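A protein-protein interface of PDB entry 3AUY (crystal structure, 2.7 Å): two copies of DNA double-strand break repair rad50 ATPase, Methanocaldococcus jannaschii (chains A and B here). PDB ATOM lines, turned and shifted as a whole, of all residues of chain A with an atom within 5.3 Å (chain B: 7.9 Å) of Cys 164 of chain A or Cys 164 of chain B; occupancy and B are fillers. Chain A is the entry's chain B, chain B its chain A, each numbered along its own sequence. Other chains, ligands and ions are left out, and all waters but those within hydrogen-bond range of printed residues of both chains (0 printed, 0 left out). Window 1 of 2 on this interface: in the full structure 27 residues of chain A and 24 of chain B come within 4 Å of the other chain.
The side-chain carboxylate of Glu 160 of chain A lies within salt-bridge range of the side-chain amino group of Lys 167 of chain B (3.7 Å).
The side-chain amino group of Lys 163 of chain B is in salt-bridge range of the side-chain carboxylate of Glu 160 of chain A (2.9 Å).
NZ of Lys 167 of chain A lies within salt-bridge range of OE1 of Glu 160 of chain B.
SG of Cys 164 of chain A is disulfide-bonded to SG of Cys 164 of chain B (2.0 Å).
OE2 of Glu 170 of chain B lies within salt-bridge range of NZ of Lys 167 of chain B (2.5 Å).
N of Lys 163 of chain B sits close to OE1 of Gln 166 of chain B, 3.5 Å away.
The backbone carbonyl oxygen (O) of Phe 224 of chain B lies within hydrogen-bond range of the side-chain amide nitrogen (NE2) of Gln 230 of chain B (2.8 Å).
Among the printed residues, pairs that only touch across the chains: Phe 161 of chain A with Lys 167 of chain B (3.2 Å), Met 168 of chain A with Phe 224 of chain B (3.2 Å), Phe 161 of chain A with Ile 171 of chain B (3.4 Å), Lys 167 of chain A with Phe 224 of chain B (3.5 Å), Met 168 of chain A with Met 168 of chain B (3.6 Å), Cys 164 of chain A with Phe 224 of chain B (3.6 Å), Cys 164 of chain A with Met 168 of chain B (3.6 Å), Phe 161 of chain A with Glu 170 of chain B (3.7 Å), Lys 167 of chain A with Phe 161 of chain B (3.9 Å), Lys 167 of chain A with Cys 164 of chain B (3.9 Å) and Met 168 of chain A with Val 220 of chain B (3.98 Å).
Of the printed residues of chain A, Phe 224 of chain B touches Cys 164 (3.6 Å), Lys 167 (3.5 Å) and Met 168 (3.2 Å).
Printed residues of chain A within 4 Å of Phe 161 of chain B: Lys 167 (3.9 Å).
Of the printed residues of chain A, Ile 171 of chain B touches Phe 161.
Printed residues of chain A within 4 Å of Glu 170 of chain B: Phe 161 (3.7 Å).
Ile 158 of chain B touches none of the printed residues of chain A.
Gly 169 of chain A touches none of the printed residues of chain B.
Printed residues of chain A that touch a printed residue of chain B: Glu 160, Phe 161, Cys 164, Lys 167 and Met 168.
Hydrophobic or aromatic side chains of chain A within 4 Å of the printed part of chain B: Phe 161 and Met 168.
Of the 19 printed residues of chain B, 10 touch a printed residue of chain A.
Glu 160 of chain A touches Lys 163 of chain B, but with the chains exchanged Lys 163 of chain A does not touch Glu 160 of chain B (6.6 Å).
Glu 160 of chain A touches Lys 167 of chain B, and with the chains exchanged Lys 167 of chain A touches Glu 160 of chain B.
Cys 164 of chain A touches its own counterpart, Cys 164 of chain B.
Lys 167 of chain A touches Cys 164 of chain B, but with the chains exchanged Cys 164 of chain A does not touch Lys 167 of chain B (4.5 Å).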
ATOM      1  N   GLU A 160      33.285 -30.890 -26.207  1.00  0.00           N
ATOM      2  CA  GLU A 160      32.874 -30.291 -24.952  1.00  0.00           C
ATOM      3  C   GLU A 160      31.778 -29.253 -25.186  1.00  0.00           C
ATOM      4  O   GLU A 160      30.900 -29.076 -24.351  1.00  0.00           O
ATOM      5  CB  GLU A 160      34.068 -29.632 -24.260  1.00  0.00           C
ATOM      6  CG  GLU A 160      34.996 -30.599 -23.533  1.00  0.00           C
ATOM      7  CD  GLU A 160      35.944 -29.885 -22.559  1.00  0.00           C
ATOM      8  OE1 GLU A 160      36.878 -29.173 -23.010  1.00  0.00           O
ATOM      9  OE2 GLU A 160      35.746 -30.033 -21.332  1.00  0.00           O
ATOM     10  N   PHE A 161      31.824 -28.567 -26.320  1.00  0.00           N
ATOM     11  CA  PHE A 161      30.813 -27.562 -26.622  1.00  0.00           C
ATOM     12  C   PHE A 161      29.507 -28.212 -27.010  1.00  0.00           C
ATOM     13  O   PHE A 161      28.443 -27.636 -26.830  1.00  0.00           O
ATOM     14  CB  PHE A 161      31.285 -26.625 -27.743  1.00  0.00           C
ATOM     15  CG  PHE A 161      32.307 -25.616 -27.290  1.00  0.00           C
ATOM     16  CD1 PHE A 161      31.961 -24.623 -26.377  1.00  0.00           C
ATOM     17  CD2 PHE A 161      33.632 -25.698 -27.720  1.00  0.00           C
ATOM     18  CE1 PHE A 161      32.921 -23.728 -25.889  1.00  0.00           C
ATOM     19  CE2 PHE A 161      34.604 -24.804 -27.237  1.00  0.00           C
ATOM     20  CZ  PHE A 161      34.244 -23.820 -26.320  1.00  0.00           C
ATOM     21  N   GLU A 162      29.581 -29.428 -27.522  1.00  0.00           N
ATOM     22  CA  GLU A 162      28.375 -30.116 -27.930  1.00  0.00           C
ATOM     23  C   GLU A 162      27.632 -30.720 -26.751  1.00  0.00           C
ATOM     24  O   GLU A 162      26.458 -31.025 -26.854  1.00  0.00           O
ATOM     25  CB  GLU A 162      28.712 -31.189 -28.955  1.00  0.00           C
ATOM     26  CG  GLU A 162      27.914 -31.049 -30.236  1.00  0.00           C
ATOM     27  CD  GLU A 162      26.461 -31.515 -30.106  1.00  0.00           C
ATOM     28  OE1 GLU A 162      25.625 -31.079 -30.934  1.00  0.00           O
ATOM     29  OE2 GLU A 162      26.155 -32.324 -29.195  1.00  0.00           O
ATOM     30  N   LYS A 163      28.309 -30.891 -25.627  1.00  0.00           N
ATOM     31  CA  LYS A 163      27.650 -31.451 -24.454  1.00  0.00           C
ATOM     32  C   LYS A 163      26.815 -30.363 -23.810  1.00  0.00           C
ATOM     33  O   LYS A 163      25.758 -30.625 -23.246  1.00  0.00           O
ATOM     34  CB  LYS A 163      28.681 -31.987 -23.461  1.00  0.00           C
ATOM     35  CG  LYS A 163      29.541 -33.081 -24.056  1.00  0.00           C
ATOM     36  CD  LYS A 163      30.560 -33.627 -23.077  1.00  0.00           C
ATOM     37  CE  LYS A 163      31.393 -34.716 -23.755  1.00  0.00           C
ATOM     38  NZ  LYS A 163      32.403 -35.327 -22.850  1.00  0.00           N
ATOM     39  N   CYS A 164      27.302 -29.133 -23.898  1.00  0.00           N
ATOM     40  CA  CYS A 164      26.594 -28.004 -23.340  1.00  0.00           C
ATOM     41  C   CYS A 164      25.409 -27.694 -24.242  1.00  0.00           C
ATOM     42  O   CYS A 164      24.425 -27.070 -23.830  1.00  0.00           O
ATOM     43  CB  CYS A 164      27.542 -26.809 -23.235  1.00  0.00           C
ATOM     44  SG  CYS A 164      28.951 -27.152 -22.133  1.00  0.00           S
ATOM     45  N   TYR A 165      25.502 -28.144 -25.487  1.00  0.00           N
ATOM     46  CA  TYR A 165      24.414 -27.937 -26.426  1.00  0.00           C
ATOM     47  C   TYR A 165      23.261 -28.804 -25.943  1.00  0.00           C
ATOM     48  O   TYR A 165      22.112 -28.378 -25.956  1.00  0.00           O
ATOM     49  CB  TYR A 165      24.838 -28.352 -27.836  1.00  0.00           C
ATOM     50  CG  TYR A 165      23.750 -28.148 -28.871  1.00  0.00           C
ATOM     51  CD1 TYR A 165      23.277 -26.866 -29.168  1.00  0.00           C
ATOM     52  CD2 TYR A 165      23.158 -29.244 -29.516  1.00  0.00           C
ATOM     53  CE1 TYR A 165      22.246 -26.672 -30.074  1.00  0.00           C
ATOM     54  CE2 TYR A 165      22.118 -29.066 -30.424  1.00  0.00           C
ATOM     55  CZ  TYR A 165      21.669 -27.775 -30.696  1.00  0.00           C
ATOM     56  OH  TYR A 165      20.639 -27.576 -31.579  1.00  0.00           O
ATOM     57  N   GLN A 166      23.575 -30.028 -25.525  1.00  0.00           N
ATOM     58  CA  GLN A 166      22.555 -30.937 -25.018  1.00  0.00           C
ATOM     59  C   GLN A 166      22.041 -30.414 -23.685  1.00  0.00           C
ATOM     60  O   GLN A 166      20.833 -30.355 -23.447  1.00  0.00           O
ATOM     61  CB  GLN A 166      23.124 -32.326 -24.796  1.00  0.00           C
ATOM     62  CG  GLN A 166      23.519 -33.074 -26.043  1.00  0.00           C
ATOM     63  CD  GLN A 166      24.140 -34.424 -25.702  1.00  0.00           C
ATOM     64  OE1 GLN A 166      23.576 -35.193 -24.904  1.00  0.00           O
ATOM     65  NE2 GLN A 166      25.303 -34.721 -26.300  1.00  0.00           N
ATOM     66  N   LYS A 167      22.968 -30.058 -22.802  1.00  0.00           N
ATOM     67  CA  LYS A 167      22.602 -29.519 -21.507  1.00  0.00           C
ATOM     68  C   LYS A 167      21.487 -28.503 -21.733  1.00  0.00           C
ATOM     69  O   LYS A 167      20.398 -28.608 -21.162  1.00  0.00           O
ATOM     70  CB  LYS A 167      23.813 -28.835 -20.884  1.00  0.00           C
ATOM     71  CG  LYS A 167      24.943 -29.785 -20.553  1.00  0.00           C
ATOM     72  CD  LYS A 167      24.565 -30.666 -19.389  1.00  0.00           C
ATOM     73  CE  LYS A 167      25.631 -31.697 -19.091  1.00  0.00           C
ATOM     74  NZ  LYS A 167      25.236 -32.558 -17.944  1.00  0.00           N
ATOM     75  N   MET A 168      21.764 -27.535 -22.600  1.00  0.00           N
ATOM     76  CA  MET A 168      20.800 -26.491 -22.913  1.00  0.00           C
ATOM     77  C   MET A 168      19.430 -27.044 -23.262  1.00  0.00           C
ATOM     78  O   MET A 168      18.416 -26.588 -22.736  1.00  0.00           O
ATOM     79  CB  MET A 168      21.302 -25.629 -24.071  1.00  0.00           C
ATOM     80  CG  MET A 168      22.468 -24.742 -23.723  1.00  0.00           C
ATOM     81  SD  MET A 168      22.881 -23.639 -25.070  1.00  0.00           S
ATOM     82  CE  MET A 168      24.649 -23.865 -25.141  1.00  0.00           C
ATOM     83  N   GLY A 169      19.394 -28.019 -24.159  1.00  0.00           N
ATOM     84  CA  GLY A 169      18.118 -28.585 -24.548  1.00  0.00           C
ATOM     85  C   GLY A 169      17.453 -29.298 -23.390  1.00  0.00           C
ATOM     86  O   GLY A 169      16.226 -29.295 -23.252  1.00  0.00           O
ATOM     87  N   ILE B 158      25.934 -31.106 -10.630  1.00  0.00           N
ATOM     88  CA  ILE B 158      26.070 -29.660 -10.546  1.00  0.00           C
ATOM     89  C   ILE B 158      27.295 -29.207 -11.339  1.00  0.00           C
ATOM     90  O   ILE B 158      27.180 -28.434 -12.277  1.00  0.00           O
ATOM     91  CB  ILE B 158      26.245 -29.182  -9.087  1.00  0.00           C
ATOM     92  CG1 ILE B 158      25.025 -29.544  -8.245  1.00  0.00           C
ATOM     93  CG2 ILE B 158      26.459 -27.692  -9.060  1.00  0.00           C
ATOM     94  CD1 ILE B 158      23.777 -28.895  -8.679  1.00  0.00           C
ATOM     95  N   ASP B 159      28.466 -29.698 -10.960  1.00  0.00           N
ATOM     96  CA  ASP B 159      29.711 -29.332 -11.625  1.00  0.00           C
ATOM     97  C   ASP B 159      29.552 -29.411 -13.126  1.00  0.00           C
ATOM     98  O   ASP B 159      30.211 -28.705 -13.870  1.00  0.00           O
ATOM     99  CB  ASP B 159      30.847 -30.250 -11.182  1.00  0.00           C
ATOM    100  CG  ASP B 159      30.569 -31.714 -11.489  1.00  0.00           C
ATOM    101  OD1 ASP B 159      31.554 -32.475 -11.635  1.00  0.00           O
ATOM    102  OD2 ASP B 159      29.376 -32.113 -11.580  1.00  0.00           O
ATOM    103  N   GLU B 160      28.669 -30.291 -13.565  1.00  0.00           N
ATOM    104  CA  GLU B 160      28.402 -30.463 -14.982  1.00  0.00           C
ATOM    105  C   GLU B 160      28.069 -29.130 -15.618  1.00  0.00           C
ATOM    106  O   GLU B 160      28.636 -28.750 -16.638  1.00  0.00           O
ATOM    107  CB  GLU B 160      27.220 -31.405 -15.161  1.00  0.00           C
ATOM    108  CG  GLU B 160      27.566 -32.828 -14.889  1.00  0.00           C
ATOM    109  CD  GLU B 160      28.352 -33.398 -16.027  1.00  0.00           C
ATOM    110  OE1 GLU B 160      27.766 -33.472 -17.131  1.00  0.00           O
ATOM    111  OE2 GLU B 160      29.539 -33.755 -15.832  1.00  0.00           O
ATOM    112  N   PHE B 161      27.129 -28.429 -14.993  1.00  0.00           N
ATOM    113  CA  PHE B 161      26.663 -27.145 -15.480  1.00  0.00           C
ATOM    114  C   PHE B 161      27.672 -26.024 -15.270  1.00  0.00           C
ATOM    115  O   PHE B 161      27.706 -25.066 -16.042  1.00  0.00           O
ATOM    116  CB  PHE B 161      25.319 -26.832 -14.825  1.00  0.00           C
ATOM    117  CG  PHE B 161      24.243 -27.797 -15.212  1.00  0.00           C
ATOM    118  CD1 PHE B 161      23.529 -27.627 -16.395  1.00  0.00           C
ATOM    119  CD2 PHE B 161      23.985 -28.928 -14.431  1.00  0.00           C
ATOM    120  CE1 PHE B 161      22.572 -28.576 -16.796  1.00  0.00           C
ATOM    121  CE2 PHE B 161      23.033 -29.876 -14.823  1.00  0.00           C
ATOM    122  CZ  PHE B 161      22.329 -29.701 -16.004  1.00  0.00           C
ATOM    123  N   GLU B 162      28.499 -26.143 -14.237  1.00  0.00           N
ATOM    124  CA  GLU B 162      29.509 -25.132 -13.975  1.00  0.00           C
ATOM    125  C   GLU B 162      30.489 -25.232 -15.124  1.00  0.00           C
ATOM    126  O   GLU B 162      30.869 -24.224 -15.706  1.00  0.00           O
ATOM    127  CB  GLU B 162      30.230 -25.402 -12.654  1.00  0.00           C
ATOM    128  CG  GLU B 162      31.162 -24.280 -12.216  1.00  0.00           C
ATOM    129  CD  GLU B 162      30.448 -22.944 -12.067  1.00  0.00           C
ATOM    130  OE1 GLU B 162      29.203 -22.935 -12.016  1.00  0.00           O
ATOM    131  OE2 GLU B 162      31.120 -21.893 -11.987  1.00  0.00           O
ATOM    132  N   LYS B 163      30.876 -26.461 -15.453  1.00  0.00           N
ATOM    133  CA  LYS B 163      31.814 -26.723 -16.544  1.00  0.00           C
ATOM    134  C   LYS B 163      31.337 -25.996 -17.798  1.00  0.00           C
ATOM    135  O   LYS B 163      32.141 -25.397 -18.502  1.00  0.00           O
ATOM    136  CB  LYS B 163      31.913 -28.235 -16.812  1.00  0.00           C
ATOM    137  CG  LYS B 163      33.302 -28.738 -17.191  1.00  0.00           C
ATOM    138  CD  LYS B 163      33.836 -28.032 -18.426  1.00  0.00           C
ATOM    139  CE  LYS B 163      35.329 -28.290 -18.650  1.00  0.00           C
ATOM    140  NZ  LYS B 163      35.847 -27.561 -19.865  1.00  0.00           N
ATOM    141  N   CYS B 164      30.033 -26.036 -18.067  1.00  0.00           N
ATOM    142  CA  CYS B 164      29.469 -25.353 -19.231  1.00  0.00           C
ATOM    143  C   CYS B 164      29.411 -23.845 -19.055  1.00  0.00           C
ATOM    144  O   CYS B 164      29.520 -23.092 -20.028  1.00  0.00           O
ATOM    145  CB  CYS B 164      28.064 -25.857 -19.536  1.00  0.00           C
ATOM    146  SG  CYS B 164      28.088 -27.485 -20.324  1.00  0.00           S
ATOM    147  N   TYR B 165      29.220 -23.407 -17.816  1.00  0.00           N
ATOM    148  CA  TYR B 165      29.179 -21.984 -17.514  1.00  0.00           C
ATOM    149  C   TYR B 165      30.514 -21.429 -17.977  1.00  0.00           C
ATOM    150  O   TYR B 165      30.585 -20.370 -18.582  1.00  0.00           O
ATOM    151  CB  TYR B 165      29.016 -21.788 -16.009  1.00  0.00           C
ATOM    152  CG  TYR B 165      29.319 -20.395 -15.502  1.00  0.00           C
ATOM    153  CD1 TYR B 165      28.339 -19.405 -15.479  1.00  0.00           C
ATOM    154  CD2 TYR B 165      30.584 -20.078 -15.011  1.00  0.00           C
ATOM    155  CE1 TYR B 165      28.610 -18.124 -14.969  1.00  0.00           C
ATOM    156  CE2 TYR B 165      30.873 -18.808 -14.501  1.00  0.00           C
ATOM    157  CZ  TYR B 165      29.884 -17.835 -14.478  1.00  0.00           C
ATOM    158  OH  TYR B 165      30.167 -16.593 -13.945  1.00  0.00           O
ATOM    159  N   GLN B 166      31.573 -22.186 -17.711  1.00  0.00           N
ATOM    160  CA  GLN B 166      32.927 -21.793 -18.070  1.00  0.00           C
ATOM    161  C   GLN B 166      33.204 -21.855 -19.576  1.00  0.00           C
ATOM    162  O   GLN B 166      33.865 -20.968 -20.126  1.00  0.00           O
ATOM    163  CB  GLN B 166      33.928 -22.642 -17.281  1.00  0.00           C
ATOM    164  CG  GLN B 166      33.917 -22.326 -15.775  1.00  0.00           C
ATOM    165  CD  GLN B 166      34.351 -23.502 -14.868  1.00  0.00           C
ATOM    166  OE1 GLN B 166      33.683 -24.547 -14.804  1.00  0.00           O
ATOM    167  NE2 GLN B 166      35.465 -23.319 -14.152  1.00  0.00           N
ATOM    168  N   LYS B 167      32.704 -22.877 -20.259  1.00  0.00           N
ATOM    169  CA  LYS B 167      32.928 -22.952 -21.698  1.00  0.00           C
ATOM    170  C   LYS B 167      32.241 -21.755 -22.349  1.00  0.00           C
ATOM    171  O   LYS B 167      32.818 -21.106 -23.216  1.00  0.00           O
ATOM    172  CB  LYS B 167      32.385 -24.267 -22.255  1.00  0.00           C
ATOM    173  CG  LYS B 167      33.163 -25.490 -21.774  1.00  0.00           C
ATOM    174  CD  LYS B 167      33.788 -26.239 -22.934  1.00  0.00           C
ATOM    175  CE  LYS B 167      34.895 -25.447 -23.607  1.00  0.00           C
ATOM    176  NZ  LYS B 167      36.191 -25.585 -22.890  1.00  0.00           N
ATOM    177  N   MET B 168      31.011 -21.462 -21.926  1.00  0.00           N
ATOM    178  CA  MET B 168      30.287 -20.316 -22.460  1.00  0.00           C
ATOM    179  C   MET B 168      31.119 -19.071 -22.214  1.00  0.00           C
ATOM    180  O   MET B 168      31.147 -18.154 -23.027  1.00  0.00           O
ATOM    181  CB  MET B 168      28.938 -20.140 -21.768  1.00  0.00           C
ATOM    182  CG  MET B 168      27.888 -21.153 -22.167  1.00  0.00           C
ATOM    183  SD  MET B 168      27.898 -21.472 -23.932  1.00  0.00           S
ATOM    184  CE  MET B 168      27.948 -23.262 -23.967  1.00  0.00           C
ATOM    185  N   GLY B 169      31.792 -19.040 -21.074  1.00  0.00           N
ATOM    186  CA  GLY B 169      32.623 -17.901 -20.757  1.00  0.00           C
ATOM    187  C   GLY B 169      33.697 -17.724 -21.809  1.00  0.00           C
ATOM    188  O   GLY B 169      34.027 -16.610 -22.191  1.00  0.00           O
ATOM    189  N   GLU B 170      34.257 -18.832 -22.273  1.00  0.00           N
ATOM    190  CA  GLU B 170      35.295 -18.777 -23.286  1.00  0.00           C
ATOM    191  C   GLU B 170      34.738 -18.011 -24.461  1.00  0.00           C
ATOM    192  O   GLU B 170      35.173 -16.897 -24.753  1.00  0.00           O
ATOM    193  CB  GLU B 170      35.687 -20.189 -23.720  1.00  0.00           C
ATOM    194  CG  GLU B 170      36.552 -20.934 -22.704  1.00  0.00           C
ATOM    195  CD  GLU B 170      36.800 -22.385 -23.091  1.00  0.00           C
ATOM    196  OE1 GLU B 170      37.083 -22.658 -24.280  1.00  0.00           O
ATOM    197  OE2 GLU B 170      36.723 -23.253 -22.197  1.00  0.00           O
ATOM    198  N   ILE B 171      33.753 -18.624 -25.108  1.00  0.00           N
ATOM    199  CA  ILE B 171      33.069 -18.062 -26.262  1.00  0.00           C
ATOM    200  C   ILE B 171      32.783 -16.583 -26.075  1.00  0.00           C
ATOM    201  O   ILE B 171      33.022 -15.783 -26.977  1.00  0.00           O
ATOM    202  CB  ILE B 171      31.744 -18.816 -26.515  1.00  0.00           C
ATOM    203  CG1 ILE B 171      32.052 -20.317 -26.669  1.00  0.00           C
ATOM    204  CG2 ILE B 171      31.029 -18.246 -27.750  1.00  0.00           C
ATOM    205  CD1 ILE B 171      30.854 -21.187 -26.893  1.00  0.00           C
ATOM    206  N   VAL B 220      22.452 -17.009 -21.341  1.00  0.00           N
ATOM    207  CA  VAL B 220      22.406 -18.452 -21.239  1.00  0.00           C
ATOM    208  C   VAL B 220      23.589 -18.915 -20.406  1.00  0.00           C
ATOM    209  O   VAL B 220      23.606 -20.035 -19.915  1.00  0.00           O
ATOM    210  CB  VAL B 220      22.395 -19.107 -22.636  1.00  0.00           C
ATOM    211  CG1 VAL B 220      23.541 -18.600 -23.440  1.00  0.00           C
ATOM    212  CG2 VAL B 220      22.477 -20.602 -22.522  1.00  0.00           C
ATOM    213  N   ARG B 221      24.571 -18.038 -20.222  1.00  0.00           N
ATOM    214  CA  ARG B 221      25.743 -18.381 -19.413  1.00  0.00           C
ATOM    215  C   ARG B 221      25.338 -18.314 -17.938  1.00  0.00           C
ATOM    216  O   ARG B 221      25.795 -19.102 -17.113  1.00  0.00           O
ATOM    217  CB  ARG B 221      26.902 -17.408 -19.701  1.00  0.00           C
ATOM    218  CG  ARG B 221      28.122 -17.573 -18.803  1.00  0.00           C
ATOM    219  CD  ARG B 221      29.232 -16.613 -19.213  1.00  0.00           C
ATOM    220  NE  ARG B 221      30.112 -16.216 -18.105  1.00  0.00           N
ATOM    221  CZ  ARG B 221      31.073 -16.972 -17.573  1.00  0.00           C
ATOM    222  NH1 ARG B 221      31.305 -18.192 -18.034  1.00  0.00           N
ATOM    223  NH2 ARG B 221      31.816 -16.502 -16.578  1.00  0.00           N
ATOM    224  N   PHE B 224      23.528 -21.461 -16.787  1.00  0.00           N
ATOM    225  CA  PHE B 224      24.335 -22.627 -16.432  1.00  0.00           C
ATOM    226  C   PHE B 224      24.946 -22.347 -15.069  1.00  0.00           C
ATOM    227  O   PHE B 224      25.280 -23.256 -14.321  1.00  0.00           O
ATOM    228  CB  PHE B 224      25.482 -22.849 -17.425  1.00  0.00           C
ATOM    229  CG  PHE B 224      25.081 -23.539 -18.690  1.00  0.00           C
ATOM    230  CD1 PHE B 224      24.557 -24.824 -18.661  1.00  0.00           C
ATOM    231  CD2 PHE B 224      25.237 -22.905 -19.919  1.00  0.00           C
ATOM    232  CE1 PHE B 224      24.188 -25.471 -19.847  1.00  0.00           C
ATOM    233  CE2 PHE B 224      24.875 -23.534 -21.108  1.00  0.00           C
ATOM    234  CZ  PHE B 224      24.347 -24.821 -21.074  1.00  0.00           C
ATOM    235  N   GLY B 225      25.074 -21.068 -14.753  1.00  0.00           N
ATOM    236  CA  GLY B 225      25.675 -20.663 -13.505  1.00  0.00           C
ATOM    237  C   GLY B 225      24.995 -20.990 -12.188  1.00  0.00           C
ATOM    238  O   GLY B 225      23.823 -21.373 -12.130  1.00  0.00           O
ATOM    239  N   GLN B 230      21.656 -24.399 -11.686  1.00  0.00           N
ATOM    240  CA  GLN B 230      22.327 -25.041 -10.554  1.00  0.00           C
ATOM    241  C   GLN B 230      21.504 -24.859  -9.286  1.00  0.00           C
ATOM    242  O   GLN B 230      21.155 -25.827  -8.611  1.00  0.00           O
ATOM    243  CB  GLN B 230      23.716 -24.454 -10.342  1.00  0.00           C
ATOM    244  CG  GLN B 230      24.656 -24.833 -11.435  1.00  0.00           C
ATOM    245  CD  GLN B 230      26.065 -24.416 -11.140  1.00  0.00           C
ATOM    246  OE1 GLN B 230      26.724 -24.978 -10.264  1.00  0.00           O
ATOM    247  NE2 GLN B 230      26.542 -23.416 -11.866  1.00  0.00           N
